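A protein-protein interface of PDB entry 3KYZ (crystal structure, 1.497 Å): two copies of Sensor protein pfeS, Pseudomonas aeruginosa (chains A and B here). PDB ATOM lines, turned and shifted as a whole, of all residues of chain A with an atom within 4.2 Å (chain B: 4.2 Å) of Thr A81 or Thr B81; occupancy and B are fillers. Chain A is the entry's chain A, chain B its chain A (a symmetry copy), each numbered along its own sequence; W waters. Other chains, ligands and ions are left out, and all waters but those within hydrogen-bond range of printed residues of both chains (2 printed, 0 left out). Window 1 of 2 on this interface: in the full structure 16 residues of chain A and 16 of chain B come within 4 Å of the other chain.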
ATOM      1  N   LEU A  64     -10.692 -15.166  -5.476  1.00  0.00           N
ATOM      2  CA  LEU A  64     -10.102 -15.401  -6.796  1.00  0.00           C
ATOM      3  C   LEU A  64      -9.328 -14.203  -7.336  1.00  0.00           C
ATOM      4  O   LEU A  64      -9.128 -14.076  -8.543  1.00  0.00           O
ATOM      5  CB  LEU A  64     -11.146 -15.906  -7.811  1.00  0.00           C
ATOM      6  CG  LEU A  64     -11.946 -17.130  -7.348  1.00  0.00           C
ATOM      7  CD1 LEU A  64     -12.942 -17.583  -8.421  1.00  0.00           C
ATOM      8  CD2 LEU A  64     -11.029 -18.288  -6.961  1.00  0.00           C
ATOM      9  N   SER A  78     -10.086 -15.349 -16.593  1.00  0.00           N
ATOM     10  CA  SER A  78     -10.814 -16.339 -17.389  1.00  0.00           C
ATOM     11  C   SER A  78     -10.187 -17.738 -17.298  1.00  0.00           C
ATOM     12  O   SER A  78     -10.852 -18.734 -17.589  1.00  0.00           O
ATOM     13  CB  SER A  78     -10.956 -15.894 -18.855  1.00  0.00           C
ATOM     14  OG  SER A  78      -9.767 -16.111 -19.606  1.00  0.00           O
ATOM     15  N   HIS A  79      -8.922 -17.811 -16.884  1.00  0.00           N
ATOM     16  CA  HIS A  79      -8.249 -19.104 -16.723  1.00  0.00           C
ATOM     17  C   HIS A  79      -8.703 -19.847 -15.472  1.00  0.00           C
ATOM     18  O   HIS A  79      -8.373 -21.018 -15.291  1.00  0.00           O
ATOM     19  CB  HIS A  79      -6.734 -18.932 -16.585  1.00  0.00           C
ATOM     20  CG  HIS A  79      -6.083 -18.200 -17.713  1.00  0.00           C
ATOM     21  ND1 HIS A  79      -4.817 -17.665 -17.610  1.00  0.00           N
ATOM     22  CD2 HIS A  79      -6.510 -17.922 -18.966  1.00  0.00           C
ATOM     23  CE1 HIS A  79      -4.495 -17.081 -18.749  1.00  0.00           C
ATOM     24  NE2 HIS A  79      -5.506 -17.219 -19.588  1.00  0.00           N
ATOM     25  N   LEU A  80      -9.412 -19.153 -14.589  1.00  0.00           N
ATOM     26  CA  LEU A  80      -9.734 -19.696 -13.276  1.00  0.00           C
ATOM     27  C   LEU A  80     -11.057 -20.447 -13.202  1.00  0.00           C
ATOM     28  O   LEU A  80     -11.425 -20.928 -12.131  1.00  0.00           O
ATOM     29  CB  LEU A  80      -9.772 -18.568 -12.245  1.00  0.00           C
ATOM     30  CG  LEU A  80      -8.492 -17.733 -12.142  1.00  0.00           C
ATOM     31  CD1 LEU A  80      -8.691 -16.627 -11.108  1.00  0.00           C
ATOM     32  CD2 LEU A  80      -7.272 -18.613 -11.809  1.00  0.00           C
ATOM     33  N   THR A  81     -11.775 -20.545 -14.316  1.00  0.00           N
ATOM     34  CA  THR A  81     -13.166 -21.001 -14.269  1.00  0.00           C
ATOM     35  C   THR A  81     -13.406 -22.452 -14.676  1.00  0.00           C
ATOM     36  O   THR A  81     -14.467 -23.005 -14.363  1.00  0.00           O
ATOM     37  CB  THR A  81     -14.078 -20.102 -15.142  1.00  0.00           C
ATOM     38  OG1 THR A  81     -13.571 -20.069 -16.482  1.00  0.00           O
ATOM     39  CG2 THR A  81     -14.132 -18.688 -14.586  1.00  0.00           C
ATOM     40  N   PHE A  82     -12.442 -23.066 -15.368  1.00  0.00           N
ATOM     41  CA  PHE A  82     -12.609 -24.424 -15.895  1.00  0.00           C
ATOM     42  C   PHE A  82     -11.392 -25.268 -15.540  1.00  0.00           C
ATOM     43  O   PHE A  82     -10.833 -25.985 -16.384  1.00  0.00           O
ATOM     44  CB  PHE A  82     -12.827 -24.412 -17.416  1.00  0.00           C
ATOM     45  CG  PHE A  82     -13.929 -23.495 -17.867  1.00  0.00           C
ATOM     46  CD1 PHE A  82     -15.239 -23.699 -17.448  1.00  0.00           C
ATOM     47  CD2 PHE A  82     -13.661 -22.444 -18.733  1.00  0.00           C
ATOM     48  CE1 PHE A  82     -16.260 -22.846 -17.868  1.00  0.00           C
ATOM     49  CE2 PHE A  82     -14.675 -21.595 -19.164  1.00  0.00           C
ATOM     50  CZ  PHE A  82     -15.977 -21.794 -18.725  1.00  0.00           C
ATOM     51  N   MET A  83     -10.988 -25.174 -14.277  1.00  0.00           N
ATOM     52  CA  MET A  83      -9.754 -25.785 -13.814  1.00  0.00           C
ATOM     53  C   MET A  83      -9.905 -27.260 -13.482  1.00  0.00           C
ATOM     54  O   MET A  83     -11.024 -27.784 -13.433  1.00  0.00           O
ATOM     55  CB  MET A  83      -9.209 -25.009 -12.614  1.00  0.00           C
ATOM     56  CG  MET A  83      -8.947 -23.542 -12.949  1.00  0.00           C
ATOM     57  SD  MET A  83      -7.786 -22.658 -11.678  1.00  0.00           S
ATOM     58  CE  MET A  83      -9.047 -22.357 -10.246  1.00  0.00           C
ATOM     59  N   ARG A 113      -4.816 -20.529  -3.164  1.00  0.00           N
ATOM     60  CA  ARG A 113      -4.413 -21.683  -3.941  1.00  0.00           C
ATOM     61  C   ARG A 113      -3.344 -21.291  -4.942  1.00  0.00           C
ATOM     62  O   ARG A 113      -3.195 -20.113  -5.294  1.00  0.00           O
ATOM     63  CB  ARG A 113      -5.615 -22.260  -4.689  1.00  0.00           C
ATOM     64  CG  ARG A 113      -6.116 -21.370  -5.821  1.00  0.00           C
ATOM     65  CD  ARG A 113      -7.384 -21.937  -6.452  1.00  0.00           C
ATOM     66  NE  ARG A 113      -8.556 -21.691  -5.613  1.00  0.00           N
ATOM     67  CZ  ARG A 113      -9.722 -22.325  -5.730  1.00  0.00           C
ATOM     68  NH1 ARG A 113      -9.884 -23.279  -6.640  1.00  0.00           N
ATOM     69  NH2 ARG A 113     -10.733 -22.004  -4.929  1.00  0.00           N
ATOM     70  N   LEU B  64     -14.627 -11.938 -12.075  1.00  0.00           N
ATOM     71  CA  LEU B  64     -15.325 -12.978 -11.315  1.00  0.00           C
ATOM     72  C   LEU B  64     -15.954 -12.464 -10.024  1.00  0.00           C
ATOM     73  O   LEU B  64     -16.209 -13.235  -9.100  1.00  0.00           O
ATOM     74  CB  LEU B  64     -14.426 -14.204 -11.060  1.00  0.00           C
ATOM     75  CG  LEU B  64     -13.779 -14.794 -12.319  1.00  0.00           C
ATOM     76  CD1 LEU B  64     -12.925 -16.021 -11.983  1.00  0.00           C
ATOM     77  CD2 LEU B  64     -14.824 -15.155 -13.372  1.00  0.00           C
ATOM     78  N   SER B  78     -15.937 -20.108  -4.625  1.00  0.00           N
ATOM     79  CA  SER B  78     -15.406 -21.453  -4.854  1.00  0.00           C
ATOM     80  C   SER B  78     -16.217 -22.232  -5.900  1.00  0.00           C
ATOM     81  O   SER B  78     -15.717 -23.203  -6.473  1.00  0.00           O
ATOM     82  CB  SER B  78     -15.293 -22.249  -3.542  1.00  0.00           C
ATOM     83  OG  SER B  78     -16.545 -22.777  -3.117  1.00  0.00           O
ATOM     84  N   HIS B  79     -17.452 -21.800  -6.157  1.00  0.00           N
ATOM     85  CA  HIS B  79     -18.288 -22.450  -7.171  1.00  0.00           C
ATOM     86  C   HIS B  79     -17.866 -22.094  -8.592  1.00  0.00           C
ATOM     87  O   HIS B  79     -18.346 -22.696  -9.551  1.00  0.00           O
ATOM     88  CB  HIS B  79     -19.752 -22.021  -7.045  1.00  0.00           C
ATOM     89  CG  HIS B  79     -20.362 -22.267  -5.704  1.00  0.00           C
ATOM     90  ND1 HIS B  79     -21.532 -21.657  -5.304  1.00  0.00           N
ATOM     91  CD2 HIS B  79     -19.979 -23.058  -4.676  1.00  0.00           C
ATOM     92  CE1 HIS B  79     -21.838 -22.056  -4.083  1.00  0.00           C
ATOM     93  NE2 HIS B  79     -20.910 -22.903  -3.677  1.00  0.00           N
ATOM     94  N   LEU B  80     -17.014 -21.085  -8.727  1.00  0.00           N
ATOM     95  CA  LEU B  80     -16.691 -20.532 -10.036  1.00  0.00           C
ATOM     96  C   LEU B  80     -15.485 -21.164 -10.717  1.00  0.00           C
ATOM     97  O   LEU B  80     -15.123 -20.753 -11.819  1.00  0.00           O
ATOM     98  CB  LEU B  80     -16.432 -19.031  -9.912  1.00  0.00           C
ATOM     99  CG  LEU B  80     -17.573 -18.218  -9.293  1.00  0.00           C
ATOM    100  CD1 LEU B  80     -17.157 -16.752  -9.198  1.00  0.00           C
ATOM    101  CD2 LEU B  80     -18.882 -18.390 -10.087  1.00  0.00           C
ATOM    102  N   THR B  81     -14.857 -22.146 -10.077  1.00  0.00           N
ATOM    103  CA  THR B  81     -13.545 -22.611 -10.527  1.00  0.00           C
ATOM    104  C   THR B  81     -13.536 -23.911 -11.328  1.00  0.00           C
ATOM    105  O   THR B  81     -12.546 -24.200 -12.011  1.00  0.00           O
ATOM    106  CB  THR B  81     -12.570 -22.778  -9.333  1.00  0.00           C
ATOM    107  OG1 THR B  81     -13.150 -23.665  -8.368  1.00  0.00           O
ATOM    108  CG2 THR B  81     -12.284 -21.436  -8.680  1.00  0.00           C
ATOM    109  N   PHE B  82     -14.618 -24.691 -11.248  1.00  0.00           N
ATOM    110  CA  PHE B  82     -14.676 -26.006 -11.894  1.00  0.00           C
ATOM    111  C   PHE B  82     -15.975 -26.139 -12.677  1.00  0.00           C
ATOM    112  O   PHE B  82     -16.681 -27.155 -12.594  1.00  0.00           O
ATOM    113  CB  PHE B  82     -14.553 -27.141 -10.866  1.00  0.00           C
ATOM    114  CG  PHE B  82     -13.363 -27.015  -9.957  1.00  0.00           C
ATOM    115  CD1 PHE B  82     -12.071 -27.028 -10.472  1.00  0.00           C
ATOM    116  CD2 PHE B  82     -13.534 -26.909  -8.583  1.00  0.00           C
ATOM    117  CE1 PHE B  82     -10.968 -26.910  -9.625  1.00  0.00           C
ATOM    118  CE2 PHE B  82     -12.439 -26.801  -7.733  1.00  0.00           C
ATOM    119  CZ  PHE B  82     -11.153 -26.795  -8.256  1.00  0.00           C
ATOM    120  N   MET B  83     -16.283 -25.095 -13.441  1.00  0.00           N
ATOM    121  CA  MET B  83     -17.560 -24.990 -14.126  1.00  0.00           C
ATOM    122  C   MET B  83     -17.598 -25.752 -15.440  1.00  0.00           C
ATOM    123  O   MET B  83     -16.562 -26.223 -15.926  1.00  0.00           O
ATOM    124  CB  MET B  83     -17.916 -23.518 -14.339  1.00  0.00           C
ATOM    125  CG  MET B  83     -17.989 -22.748 -13.023  1.00  0.00           C
ATOM    126  SD  MET B  83     -18.934 -21.065 -13.167  1.00  0.00           S
ATOM    127  CE  MET B  83     -17.557 -19.993 -13.996  1.00  0.00           C
ATOM    128  N   ARG B 113     -21.045 -12.998 -17.207  1.00  0.00           N
ATOM    129  CA  ARG B 113     -21.653 -14.280 -17.498  1.00  0.00           C
ATOM    130  C   ARG B 113     -22.716 -14.601 -16.466  1.00  0.00           C
ATOM    131  O   ARG B 113     -22.719 -14.051 -15.356  1.00  0.00           O
ATOM    132  CB  ARG B 113     -20.592 -15.381 -17.487  1.00  0.00           C
ATOM    133  CG  ARG B 113     -20.042 -15.685 -16.098  1.00  0.00           C
ATOM    134  CD  ARG B 113     -18.907 -16.704 -16.163  1.00  0.00           C
ATOM    135  NE  ARG B 113     -17.663 -16.090 -16.625  1.00  0.00           N
ATOM    136  CZ  ARG B 113     -16.607 -16.762 -17.081  1.00  0.00           C
ATOM    137  NH1 ARG B 113     -16.637 -18.088 -17.171  1.00  0.00           N
ATOM    138  NH2 ARG B 113     -15.514 -16.104 -17.452  1.00  0.00           N
HETATM  139  O   HOH W   1     -12.751 -23.846  -5.576  1.00  0.00           O
HETATM  140  O   HOH W   2     -13.818 -18.090 -18.485  1.00  0.00           O
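O of Thr B81 lies close to O of Thr A81 (3.3 Å). The backbone carbonyl oxygen of Leu A80 lies close to the backbone carbonyl oxygen of Thr B81 (3.5 Å). O of Thr B81 is in hydrogen-bond range of N of Met A83. O of Thr A81 sits close to O of Leu B80 (3.5 Å). N of Met B83 is in hydrogen-bond range of O of Thr A81 (2.9 Å).
O of Ser B78 sits at hydrogen-bond distance from OG1 of Thr B81 (3.2 Å). The side-chain hydroxyl (OG1) of Thr A81 sits at hydrogen-bond distance from the backbone carbonyl oxygen (O) of Ser A78 (3.2 Å).
Among the printed residues, pairs that only touch across the chains: Met A83 with Phe B82, Phe A82 with Met B83, Phe A82 with Thr B81, Thr A81 with Phe B82, Thr A81 with Arg B113, Arg A113 with Thr B81, Leu A80 with Leu B80, Thr A81 with Leu B64, Leu A64 with Thr B81 and Leu A64 with Leu B64.
Thr A81 touches just these residues of chain B: Leu B64 (3.8 Å), Leu B80 (3.1 Å), Thr B81 (3.3 Å), Phe B82 (3.5 Å), Met B83 (2.9 Å) and Arg B113 (3.6 Å). Of the printed residues of chain B, Phe A82 touches Thr B81 (3.5 Å) and Met B83 (3.2 Å). Of the printed residues of chain B, Met A83 touches Thr B81 and Phe B82. Thr B81 touches just these residues of chain A: Leu A64 (3.8 Å), Leu A80 (3.1 Å), Thr A81 (3.3 Å), Phe A82 (3.5 Å), Met A83 (2.9 Å) and Arg A113 (3.6 Å). The nearest printed residue of chain B that does not touch Leu A64 is Leu B80 (4.1 Å).
Of the 8 printed residues of chain A, 6 touch a printed residue of chain B. Of the 8 printed residues of chain B, 6 touch a printed residue of chain A. Among the printed residues, 15 pairs touch across the chains. Among the printed residues, no Asp or Glu carboxylate lies within 4 Å of a Lys or Arg side-chain nitrogen of the other chain.
Leu B64 touches its own counterpart, Leu A64. Thr A81 touches Phe B82, and with the chains exchanged Phe A82 touches Thr B81. Thr A81 touches Met B83, and with the chains exchanged Met A83 touches Thr B81. Thr A81 touches Arg B113, and with the chains exchanged Arg A113 touches Thr B81.
Water W1 lies within hydrogen-bond range of the guanidinium group of Arg A113 (2.8 Å), the side-chain hydroxyl of Thr B81 (2.8 Å) and the backbone carbonyl oxygen of Ser B78 (3.2 Å). Water W2 lies within hydrogen-bond range of the guanidinium group (NH2) of Arg B113 (2.8 Å), the side-chain hydroxyl (OG1) of Thr A81 (2.8 Å) and the backbone carbonyl oxygen (O) of Ser A78 (3.2 Å).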
